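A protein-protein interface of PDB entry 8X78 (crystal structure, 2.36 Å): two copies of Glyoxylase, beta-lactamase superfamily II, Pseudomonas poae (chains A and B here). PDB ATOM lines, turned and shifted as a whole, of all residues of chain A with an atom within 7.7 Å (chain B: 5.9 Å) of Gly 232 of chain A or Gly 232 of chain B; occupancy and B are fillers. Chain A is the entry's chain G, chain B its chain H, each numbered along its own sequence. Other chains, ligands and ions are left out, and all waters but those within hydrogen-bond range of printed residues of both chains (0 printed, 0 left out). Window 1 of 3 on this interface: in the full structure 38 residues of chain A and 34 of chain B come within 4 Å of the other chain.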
ATOM      1  N   LYS A  27      -7.628 -16.829 -15.379  1.00  0.00           N
ATOM      2  CA  LYS A  27      -8.462 -16.438 -14.251  1.00  0.00           C
ATOM      3  C   LYS A  27      -9.929 -16.763 -14.517  1.00  0.00           C
ATOM      4  O   LYS A  27     -10.640 -17.210 -13.609  1.00  0.00           O
ATOM      5  CB  LYS A  27      -8.289 -14.948 -13.956  1.00  0.00           C
ATOM      6  CG  LYS A  27      -6.930 -14.533 -13.403  1.00  0.00           C
ATOM      7  CD  LYS A  27      -6.922 -13.030 -13.152  1.00  0.00           C
ATOM      8  CE  LYS A  27      -5.586 -12.532 -12.653  1.00  0.00           C
ATOM      9  NZ  LYS A  27      -4.576 -12.708 -13.730  1.00  0.00           N
ATOM     10  N   ASP A  28     -10.394 -16.601 -15.762  1.00  0.00           N
ATOM     11  CA  ASP A  28     -11.810 -16.869 -16.021  1.00  0.00           C
ATOM     12  C   ASP A  28     -12.150 -18.323 -15.725  1.00  0.00           C
ATOM     13  O   ASP A  28     -13.278 -18.626 -15.323  1.00  0.00           O
ATOM     14  CB  ASP A  28     -12.207 -16.492 -17.466  1.00  0.00           C
ATOM     15  CG  ASP A  28     -11.404 -17.238 -18.536  1.00  0.00           C
ATOM     16  OD1 ASP A  28     -11.824 -18.344 -18.963  1.00  0.00           O
ATOM     17  OD2 ASP A  28     -10.367 -16.704 -18.968  1.00  0.00           O
ATOM     18  N   PHE A  29     -11.174 -19.220 -15.869  1.00  0.00           N
ATOM     19  CA  PHE A  29     -11.367 -20.624 -15.518  1.00  0.00           C
ATOM     20  C   PHE A  29     -11.968 -20.786 -14.122  1.00  0.00           C
ATOM     21  O   PHE A  29     -12.996 -21.458 -13.950  1.00  0.00           O
ATOM     22  CB  PHE A  29     -10.024 -21.355 -15.609  1.00  0.00           C
ATOM     23  CG  PHE A  29     -10.138 -22.852 -15.585  1.00  0.00           C
ATOM     24  CD1 PHE A  29     -10.181 -23.534 -14.376  1.00  0.00           C
ATOM     25  CD2 PHE A  29     -10.194 -23.580 -16.764  1.00  0.00           C
ATOM     26  CE1 PHE A  29     -10.280 -24.917 -14.345  1.00  0.00           C
ATOM     27  CE2 PHE A  29     -10.295 -24.958 -16.737  1.00  0.00           C
ATOM     28  CZ  PHE A  29     -10.331 -25.629 -15.530  1.00  0.00           C
ATOM     29  N   PHE A  30     -11.336 -20.178 -13.110  1.00  0.00           N
ATOM     30  CA  PHE A  30     -11.759 -20.330 -11.716  1.00  0.00           C
ATOM     31  C   PHE A  30     -12.776 -19.287 -11.262  1.00  0.00           C
ATOM     32  O   PHE A  30     -13.654 -19.607 -10.447  1.00  0.00           O
ATOM     33  CB  PHE A  30     -10.546 -20.251 -10.772  1.00  0.00           C
ATOM     34  CG  PHE A  30      -9.600 -21.412 -10.885  1.00  0.00           C
ATOM     35  CD1 PHE A  30     -10.049 -22.706 -10.675  1.00  0.00           C
ATOM     36  CD2 PHE A  30      -8.264 -21.210 -11.196  1.00  0.00           C
ATOM     37  CE1 PHE A  30      -9.187 -23.784 -10.770  1.00  0.00           C
ATOM     38  CE2 PHE A  30      -7.384 -22.283 -11.304  1.00  0.00           C
ATOM     39  CZ  PHE A  30      -7.846 -23.577 -11.084  1.00  0.00           C
ATOM     40  N   GLY A  31     -12.697 -18.067 -11.789  1.00  0.00           N
ATOM     41  CA  GLY A  31     -13.405 -16.942 -11.208  1.00  0.00           C
ATOM     42  C   GLY A  31     -14.689 -16.521 -11.898  1.00  0.00           C
ATOM     43  O   GLY A  31     -15.528 -15.859 -11.282  1.00  0.00           O
ATOM     44  N   GLY A  32     -14.850 -16.887 -13.169  1.00  0.00           N
ATOM     45  CA  GLY A  32     -16.064 -16.593 -13.918  1.00  0.00           C
ATOM     46  C   GLY A  32     -15.809 -15.966 -15.274  1.00  0.00           C
ATOM     47  O   GLY A  32     -14.934 -15.105 -15.415  1.00  0.00           O
ATOM     48  N   ALA A  33     -16.597 -16.361 -16.278  1.00  0.00           N
ATOM     49  CA  ALA A  33     -16.440 -15.805 -17.617  1.00  0.00           C
ATOM     50  C   ALA A  33     -16.813 -14.336 -17.687  1.00  0.00           C
ATOM     51  O   ALA A  33     -16.477 -13.668 -18.674  1.00  0.00           O
ATOM     52  CB  ALA A  33     -17.281 -16.581 -18.632  1.00  0.00           C
ATOM     53  N   GLY A  34     -17.501 -13.809 -16.689  1.00  0.00           N
ATOM     54  CA  GLY A  34     -17.827 -12.398 -16.777  1.00  0.00           C
ATOM     55  C   GLY A  34     -16.740 -11.526 -16.182  1.00  0.00           C
ATOM     56  O   GLY A  34     -15.998 -10.836 -16.891  1.00  0.00           O
ATOM     57  N   TRP A 152     -13.809 -32.351 -23.654  1.00  0.00           N
ATOM     58  CA  TRP A 152     -14.396 -31.634 -22.523  1.00  0.00           C
ATOM     59  C   TRP A 152     -14.799 -32.575 -21.396  1.00  0.00           C
ATOM     60  O   TRP A 152     -14.577 -32.268 -20.219  1.00  0.00           O
ATOM     61  CB  TRP A 152     -15.594 -30.803 -22.970  1.00  0.00           C
ATOM     62  CG  TRP A 152     -16.191 -30.040 -21.838  1.00  0.00           C
ATOM     63  CD1 TRP A 152     -15.833 -28.800 -21.393  1.00  0.00           C
ATOM     64  CD2 TRP A 152     -17.225 -30.501 -20.964  1.00  0.00           C
ATOM     65  NE1 TRP A 152     -16.607 -28.447 -20.313  1.00  0.00           N
ATOM     66  CE2 TRP A 152     -17.462 -29.480 -20.025  1.00  0.00           C
ATOM     67  CE3 TRP A 152     -17.983 -31.675 -20.896  1.00  0.00           C
ATOM     68  CZ2 TRP A 152     -18.438 -29.590 -19.035  1.00  0.00           C
ATOM     69  CZ3 TRP A 152     -18.929 -31.794 -19.914  1.00  0.00           C
ATOM     70  CH2 TRP A 152     -19.163 -30.751 -18.997  1.00  0.00           C
ATOM     71  N   TYR A 220     -14.330 -22.821  -6.111  1.00  0.00           N
ATOM     72  CA  TYR A 220     -12.937 -22.708  -6.539  1.00  0.00           C
ATOM     73  C   TYR A 220     -12.222 -21.611  -5.759  1.00  0.00           C
ATOM     74  O   TYR A 220     -11.124 -21.809  -5.225  1.00  0.00           O
ATOM     75  CB  TYR A 220     -12.890 -22.360  -8.023  1.00  0.00           C
ATOM     76  CG  TYR A 220     -12.953 -23.474  -9.034  1.00  0.00           C
ATOM     77  CD1 TYR A 220     -12.371 -24.700  -8.805  1.00  0.00           C
ATOM     78  CD2 TYR A 220     -13.590 -23.267 -10.254  1.00  0.00           C
ATOM     79  CE1 TYR A 220     -12.419 -25.698  -9.771  1.00  0.00           C
ATOM     80  CE2 TYR A 220     -13.645 -24.251 -11.218  1.00  0.00           C
ATOM     81  CZ  TYR A 220     -13.061 -25.463 -10.975  1.00  0.00           C
ATOM     82  OH  TYR A 220     -13.130 -26.441 -11.944  1.00  0.00           O
ATOM     83  N   ASN A 224     -15.932 -16.635  -5.868  1.00  0.00           N
ATOM     84  CA  ASN A 224     -17.133 -17.349  -6.291  1.00  0.00           C
ATOM     85  C   ASN A 224     -18.276 -17.142  -5.312  1.00  0.00           C
ATOM     86  O   ASN A 224     -19.403 -16.816  -5.708  1.00  0.00           O
ATOM     87  CB  ASN A 224     -16.871 -18.846  -6.447  1.00  0.00           C
ATOM     88  CG  ASN A 224     -15.957 -19.160  -7.579  1.00  0.00           C
ATOM     89  OD1 ASN A 224     -15.166 -20.095  -7.508  1.00  0.00           O
ATOM     90  ND2 ASN A 224     -16.067 -18.399  -8.646  1.00  0.00           N
ATOM     91  N   TRP A 229     -20.892 -15.757  -8.068  1.00  0.00           N
ATOM     92  CA  TRP A 229     -20.580 -15.797  -9.496  1.00  0.00           C
ATOM     93  C   TRP A 229     -19.901 -17.130  -9.764  1.00  0.00           C
ATOM     94  O   TRP A 229     -18.698 -17.281  -9.502  1.00  0.00           O
ATOM     95  CB  TRP A 229     -19.683 -14.635  -9.918  1.00  0.00           C
ATOM     96  CG  TRP A 229     -19.731 -14.341 -11.392  1.00  0.00           C
ATOM     97  CD1 TRP A 229     -19.379 -15.170 -12.415  1.00  0.00           C
ATOM     98  CD2 TRP A 229     -20.183 -13.121 -12.000  1.00  0.00           C
ATOM     99  NE1 TRP A 229     -19.574 -14.542 -13.626  1.00  0.00           N
ATOM    100  CE2 TRP A 229     -20.073 -13.285 -13.397  1.00  0.00           C
ATOM    101  CE3 TRP A 229     -20.663 -11.906 -11.497  1.00  0.00           C
ATOM    102  CZ2 TRP A 229     -20.426 -12.275 -14.301  1.00  0.00           C
ATOM    103  CZ3 TRP A 229     -21.016 -10.903 -12.393  1.00  0.00           C
ATOM    104  CH2 TRP A 229     -20.891 -11.095 -13.779  1.00  0.00           C
ATOM    105  N   PRO A 230     -20.629 -18.109 -10.298  1.00  0.00           N
ATOM    106  CA  PRO A 230     -20.064 -19.444 -10.479  1.00  0.00           C
ATOM    107  C   PRO A 230     -18.919 -19.411 -11.477  1.00  0.00           C
ATOM    108  O   PRO A 230     -18.815 -18.473 -12.279  1.00  0.00           O
ATOM    109  CB  PRO A 230     -21.251 -20.264 -11.013  1.00  0.00           C
ATOM    110  CG  PRO A 230     -22.237 -19.276 -11.510  1.00  0.00           C
ATOM    111  CD  PRO A 230     -22.030 -18.006 -10.754  1.00  0.00           C
ATOM    112  N   PRO A 231     -18.042 -20.416 -11.466  1.00  0.00           N
ATOM    113  CA  PRO A 231     -16.806 -20.338 -12.258  1.00  0.00           C
ATOM    114  C   PRO A 231     -17.078 -20.491 -13.748  1.00  0.00           C
ATOM    115  O   PRO A 231     -18.161 -20.892 -14.178  1.00  0.00           O
ATOM    116  CB  PRO A 231     -15.964 -21.509 -11.735  1.00  0.00           C
ATOM    117  CG  PRO A 231     -16.644 -21.970 -10.471  1.00  0.00           C
ATOM    118  CD  PRO A 231     -18.093 -21.639 -10.648  1.00  0.00           C
ATOM    119  N   GLY A 232     -16.051 -20.168 -14.547  1.00  0.00           N
ATOM    120  CA  GLY A 232     -16.144 -20.343 -15.991  1.00  0.00           C
ATOM    121  C   GLY A 232     -16.027 -21.788 -16.446  1.00  0.00           C
ATOM    122  O   GLY A 232     -16.565 -22.158 -17.496  1.00  0.00           O
ATOM    123  N   TYR A 233     -15.332 -22.625 -15.670  1.00  0.00           N
ATOM    124  CA  TYR A 233     -15.237 -24.052 -15.930  1.00  0.00           C
ATOM    125  C   TYR A 233     -15.848 -24.780 -14.744  1.00  0.00           C
ATOM    126  O   TYR A 233     -15.471 -24.529 -13.595  1.00  0.00           O
ATOM    127  CB  TYR A 233     -13.787 -24.505 -16.160  1.00  0.00           C
ATOM    128  CG  TYR A 233     -13.679 -26.022 -16.213  1.00  0.00           C
ATOM    129  CD1 TYR A 233     -13.963 -26.717 -17.381  1.00  0.00           C
ATOM    130  CD2 TYR A 233     -13.354 -26.757 -15.079  1.00  0.00           C
ATOM    131  CE1 TYR A 233     -13.910 -28.089 -17.433  1.00  0.00           C
ATOM    132  CE2 TYR A 233     -13.284 -28.136 -15.116  1.00  0.00           C
ATOM    133  CZ  TYR A 233     -13.561 -28.798 -16.295  1.00  0.00           C
ATOM    134  OH  TYR A 233     -13.490 -30.173 -16.331  1.00  0.00           O
ATOM    135  N   HIS A 234     -16.827 -25.631 -15.023  1.00  0.00           N
ATOM    136  CA  HIS A 234     -17.407 -26.565 -14.067  1.00  0.00           C
ATOM    137  C   HIS A 234     -18.207 -27.550 -14.908  1.00  0.00           C
ATOM    138  O   HIS A 234     -18.435 -27.322 -16.097  1.00  0.00           O
ATOM    139  CB  HIS A 234     -18.281 -25.866 -13.021  1.00  0.00           C
ATOM    140  CG  HIS A 234     -19.522 -25.257 -13.595  1.00  0.00           C
ATOM    141  ND1 HIS A 234     -20.669 -25.985 -13.836  1.00  0.00           N
ATOM    142  CD2 HIS A 234     -19.770 -24.006 -14.048  1.00  0.00           C
ATOM    143  CE1 HIS A 234     -21.587 -25.199 -14.371  1.00  0.00           C
ATOM    144  NE2 HIS A 234     -21.065 -23.992 -14.512  1.00  0.00           N
ATOM    145  N   GLN A 235     -18.604 -28.656 -14.303  1.00  0.00           N
ATOM    146  CA  GLN A 235     -19.297 -29.689 -15.060  1.00  0.00           C
ATOM    147  C   GLN A 235     -20.653 -30.022 -14.456  1.00  0.00           C
ATOM    148  O   GLN A 235     -21.072 -31.178 -14.428  1.00  0.00           O
ATOM    149  CB  GLN A 235     -18.416 -30.925 -15.197  1.00  0.00           C
ATOM    150  CG  GLN A 235     -17.073 -30.562 -15.855  1.00  0.00           C
ATOM    151  CD  GLN A 235     -16.288 -31.780 -16.328  1.00  0.00           C
ATOM    152  OE1 GLN A 235     -15.810 -32.582 -15.519  1.00  0.00           O
ATOM    153  NE2 GLN A 235     -16.137 -31.911 -17.644  1.00  0.00           N
ATOM    154  N   ALA A 238     -24.965 -24.239 -12.993  1.00  0.00           N
ATOM    155  CA  ALA A 238     -24.489 -23.008 -12.376  1.00  0.00           C
ATOM    156  C   ALA A 238     -25.461 -22.512 -11.308  1.00  0.00           C
ATOM    157  O   ALA A 238     -25.037 -22.049 -10.242  1.00  0.00           O
ATOM    158  CB  ALA A 238     -24.262 -21.948 -13.447  1.00  0.00           C
ATOM    159  N   GLN A 241     -25.075 -24.304  -8.065  1.00  0.00           N
ATOM    160  CA  GLN A 241     -23.988 -23.742  -7.270  1.00  0.00           C
ATOM    161  C   GLN A 241     -24.447 -22.497  -6.519  1.00  0.00           C
ATOM    162  O   GLN A 241     -24.081 -22.294  -5.352  1.00  0.00           O
ATOM    163  CB  GLN A 241     -22.789 -23.446  -8.167  1.00  0.00           C
ATOM    164  CG  GLN A 241     -22.116 -24.707  -8.676  1.00  0.00           C
ATOM    165  CD  GLN A 241     -21.060 -24.428  -9.726  1.00  0.00           C
ATOM    166  OE1 GLN A 241     -21.189 -24.843 -10.877  1.00  0.00           O
ATOM    167  NE2 GLN A 241     -20.017 -23.714  -9.337  1.00  0.00           N
ATOM    168  N   ASP B  28     -14.139 -16.474 -24.353  1.00  0.00           N
ATOM    169  CA  ASP B  28     -14.459 -17.599 -23.472  1.00  0.00           C
ATOM    170  C   ASP B  28     -15.909 -17.579 -22.996  1.00  0.00           C
ATOM    171  O   ASP B  28     -16.440 -18.627 -22.598  1.00  0.00           O
ATOM    172  CB  ASP B  28     -13.517 -17.621 -22.266  1.00  0.00           C
ATOM    173  CG  ASP B  28     -13.538 -16.328 -21.474  1.00  0.00           C
ATOM    174  OD1 ASP B  28     -14.456 -16.142 -20.656  1.00  0.00           O
ATOM    175  OD2 ASP B  28     -12.615 -15.502 -21.658  1.00  0.00           O
ATOM    176  N   PHE B  29     -16.540 -16.405 -23.010  1.00  0.00           N
ATOM    177  CA  PHE B  29     -17.959 -16.251 -22.714  1.00  0.00           C
ATOM    178  C   PHE B  29     -18.806 -17.174 -23.591  1.00  0.00           C
ATOM    179  O   PHE B  29     -19.585 -17.996 -23.093  1.00  0.00           O
ATOM    180  CB  PHE B  29     -18.322 -14.776 -22.937  1.00  0.00           C
ATOM    181  CG  PHE B  29     -19.662 -14.358 -22.395  1.00  0.00           C
ATOM    182  CD1 PHE B  29     -20.812 -14.472 -23.172  1.00  0.00           C
ATOM    183  CD2 PHE B  29     -19.762 -13.786 -21.135  1.00  0.00           C
ATOM    184  CE1 PHE B  29     -22.048 -14.052 -22.689  1.00  0.00           C
ATOM    185  CE2 PHE B  29     -20.994 -13.365 -20.646  1.00  0.00           C
ATOM    186  CZ  PHE B  29     -22.139 -13.498 -21.428  1.00  0.00           C
ATOM    187  N   PHE B  30     -18.658 -17.044 -24.910  1.00  0.00           N
ATOM    188  CA  PHE B  30     -19.445 -17.807 -25.873  1.00  0.00           C
ATOM    189  C   PHE B  30     -18.833 -19.156 -26.224  1.00  0.00           C
ATOM    190  O   PHE B  30     -19.574 -20.090 -26.554  1.00  0.00           O
ATOM    191  CB  PHE B  30     -19.622 -17.004 -27.168  1.00  0.00           C
ATOM    192  CG  PHE B  30     -20.489 -15.798 -27.020  1.00  0.00           C
ATOM    193  CD1 PHE B  30     -21.732 -15.894 -26.410  1.00  0.00           C
ATOM    194  CD2 PHE B  30     -20.063 -14.558 -27.489  1.00  0.00           C
ATOM    195  CE1 PHE B  30     -22.547 -14.774 -26.272  1.00  0.00           C
ATOM    196  CE2 PHE B  30     -20.867 -13.433 -27.352  1.00  0.00           C
ATOM    197  CZ  PHE B  30     -22.109 -13.541 -26.743  1.00  0.00           C
ATOM    198  N   GLY B  31     -17.505 -19.276 -26.173  1.00  0.00           N
ATOM    199  CA  GLY B  31     -16.820 -20.436 -26.717  1.00  0.00           C
ATOM    200  C   GLY B  31     -16.323 -21.449 -25.704  1.00  0.00           C
ATOM    201  O   GLY B  31     -16.134 -22.624 -26.043  1.00  0.00           O
ATOM    202  N   GLY B  32     -16.103 -21.007 -24.467  1.00  0.00           N
ATOM    203  CA  GLY B  32     -15.748 -21.905 -23.382  1.00  0.00           C
ATOM    204  C   GLY B  32     -14.457 -21.568 -22.664  1.00  0.00           C
ATOM    205  O   GLY B  32     -13.465 -21.219 -23.305  1.00  0.00           O
ATOM    206  N   ALA B  33     -14.457 -21.665 -21.336  1.00  0.00           N
ATOM    207  CA  ALA B  33     -13.213 -21.592 -20.580  1.00  0.00           C
ATOM    208  C   ALA B  33     -12.281 -22.728 -20.982  1.00  0.00           C
ATOM    209  O   ALA B  33     -12.718 -23.832 -21.314  1.00  0.00           O
ATOM    210  CB  ALA B  33     -13.482 -21.664 -19.075  1.00  0.00           C
ATOM    211  N   PRO B 230     -19.154 -26.899 -23.767  1.00  0.00           N
ATOM    212  CA  PRO B 230     -20.117 -25.887 -23.308  1.00  0.00           C
ATOM    213  C   PRO B 230     -19.430 -24.557 -23.047  1.00  0.00           C
ATOM    214  O   PRO B 230     -18.220 -24.515 -22.770  1.00  0.00           O
ATOM    215  CB  PRO B 230     -20.697 -26.491 -22.019  1.00  0.00           C
ATOM    216  CG  PRO B 230     -19.700 -27.579 -21.603  1.00  0.00           C
ATOM    217  CD  PRO B 230     -19.005 -28.039 -22.840  1.00  0.00           C
ATOM    218  N   PRO B 231     -20.173 -23.452 -23.152  1.00  0.00           N
ATOM    219  CA  PRO B 231     -19.567 -22.115 -23.045  1.00  0.00           C
ATOM    220  C   PRO B 231     -19.127 -21.789 -21.624  1.00  0.00           C
ATOM    221  O   PRO B 231     -19.495 -22.452 -20.652  1.00  0.00           O
ATOM    222  CB  PRO B 231     -20.698 -21.174 -23.491  1.00  0.00           C
ATOM    223  CG  PRO B 231     -21.723 -22.051 -24.165  1.00  0.00           C
ATOM    224  CD  PRO B 231     -21.576 -23.409 -23.603  1.00  0.00           C
ATOM    225  N   GLY B 232     -18.358 -20.699 -21.512  1.00  0.00           N
ATOM    226  CA  GLY B 232     -17.846 -20.268 -20.215  1.00  0.00           C
ATOM    227  C   GLY B 232     -18.850 -19.520 -19.359  1.00  0.00           C
ATOM    228  O   GLY B 232     -18.708 -19.470 -18.130  1.00  0.00           O
ATOM    229  N   TYR B 233     -19.846 -18.901 -19.986  1.00  0.00           N
ATOM    230  CA  TYR B 233     -20.989 -18.318 -19.302  1.00  0.00           C
ATOM    231  C   TYR B 233     -22.230 -19.059 -19.757  1.00  0.00           C
ATOM    232  O   TYR B 233     -22.441 -19.239 -20.959  1.00  0.00           O
ATOM    233  CB  TYR B 233     -21.136 -16.818 -19.599  1.00  0.00           C
ATOM    234  CG  TYR B 233     -22.471 -16.242 -19.130  1.00  0.00           C
ATOM    235  CD1 TYR B 233     -22.640 -15.827 -17.816  1.00  0.00           C
ATOM    236  CD2 TYR B 233     -23.557 -16.136 -19.994  1.00  0.00           C
ATOM    237  CE1 TYR B 233     -23.830 -15.324 -17.367  1.00  0.00           C
ATOM    238  CE2 TYR B 233     -24.775 -15.627 -19.555  1.00  0.00           C
ATOM    239  CZ  TYR B 233     -24.907 -15.219 -18.235  1.00  0.00           C
ATOM    240  OH  TYR B 233     -26.109 -14.702 -17.769  1.00  0.00           O
ATOM    241  N   HIS B 234     -23.025 -19.509 -18.802  1.00  0.00           N
ATOM    242  CA  HIS B 234     -24.366 -20.012 -19.069  1.00  0.00           C
ATOM    243  C   HIS B 234     -25.046 -20.141 -17.716  1.00  0.00           C
ATOM    244  O   HIS B 234     -24.432 -19.914 -16.669  1.00  0.00           O
ATOM    245  CB  HIS B 234     -24.342 -21.331 -19.846  1.00  0.00           C
ATOM    246  CG  HIS B 234     -23.784 -22.481 -19.071  1.00  0.00           C
ATOM    247  ND1 HIS B 234     -24.474 -23.095 -18.044  1.00  0.00           N
ATOM    248  CD2 HIS B 234     -22.599 -23.131 -19.168  1.00  0.00           C
ATOM    249  CE1 HIS B 234     -23.739 -24.073 -17.544  1.00  0.00           C
ATOM    250  NE2 HIS B 234     -22.598 -24.115 -18.210  1.00  0.00           N
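Asp 28 of chain A touches Ala 33 of chain B, and with the chains exchanged Ala 33 of chain A touches Asp 28 of chain B.
Ala 33 of chain A touches Tyr 233 of chain B, and with the chains exchanged Tyr 233 of chain A touches Ala 33 of chain B.
Gly 232 of chain A touches its own counterpart, Gly 232 of chain B.
His 234 of chain B touches its own counterpart, His 234 of chain A.
Of the 11 pairs that touch across the chains among the printed residues, 9 have their exchanged pair printed and touching as well.
Asp 28 of chain A touches Asp 28 of chain B.
OD1 of Asp 28 of chain A touches CB of Ala 33 of chain B, 3.7 Å away.
Asp 28 of chain B touches Ala 33 of chain A (OD1 to CB, 3.5 Å).
CB of Ala 33 of chain A touches O of Gly 232 of chain B (3.3 Å).
N of Tyr 233 of chain B touches CB of Ala 33 of chain A, 3.7 Å away.
CG of Pro 230 of chain B touches CE2 of Trp 152 of chain A (3.3 Å).
Gly 232 of chain A touches Ala 33 of chain B.
Tyr 233 of chain A touches Ala 33 of chain B (N to CB, 3.99 Å).
His 234 of chain B touches His 234 of chain A.
His 234 of chain B touches Ala 238 of chain A (O to CB, 3.8 Å).
The backbone carbonyl oxygen (O) of Gly 232 of chain A lies close to the backbone carbonyl oxygen (O) of Gly 232 of chain B.
Of chain B, only Ala 33 and Gly 232 come within 4 Å of Gly 232 of chain A.
Of the printed residues of chain B, Tyr 233 of chain A touches Ala 33 (3.99 Å).
Of the printed residues of chain B, Ala 238 of chain A touches His 234 (3.8 Å).
Gly 232 of chain B touches just these residues of chain A: Ala 33 and Gly 232.
Of the printed residues of chain A, His 234 of chain B touches His 234 and Ala 238.
The backbone carbonyl oxygen of Phe 29 of chain B is in hydrogen-bond range of the backbone NH of Tyr 233 of chain B.
The backbone carbonyl oxygen (O) of Asp 28 of chain B is in hydrogen-bond range of the backbone NH (N) of Gly 232 of chain B.
The side-chain hydroxyl (OH) of Tyr 220 of chain A sits close to the backbone carbonyl oxygen (O) of Tyr 233 of chain A, at 3.4 Å.
The backbone NH (N) of Gly 232 of chain A is in hydrogen-bond range of the backbone carbonyl oxygen (O) of Phe 29 of chain A.
The side-chain amide nitrogen of Gln 235 of chain A sits close to the side-chain hydroxyl of Tyr 233 of chain A (3.4 Å).
O of Trp 152 of chain A lies within hydrogen-bond range of NE2 of Gln 235 of chain A (3.0 Å).
Of the 11 printed residues of chain B, 6 touch a printed residue of chain A.
Hydrophobic or aromatic side chains of chain B that line the printed part of chain A: Ala 33, Pro 230, Tyr 233 and His 234.
Hydrophobic or aromatic side chains of chain A that line the printed part of chain B: Ala 33, Trp 152, His 234 and Ala 238.
Among the printed residues, 11 pairs touch across the chains.
Among the printed residues, no Asp or Glu carboxylate lies within 4 Å of a Lys or Arg side-chain nitrogen of the other chain.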
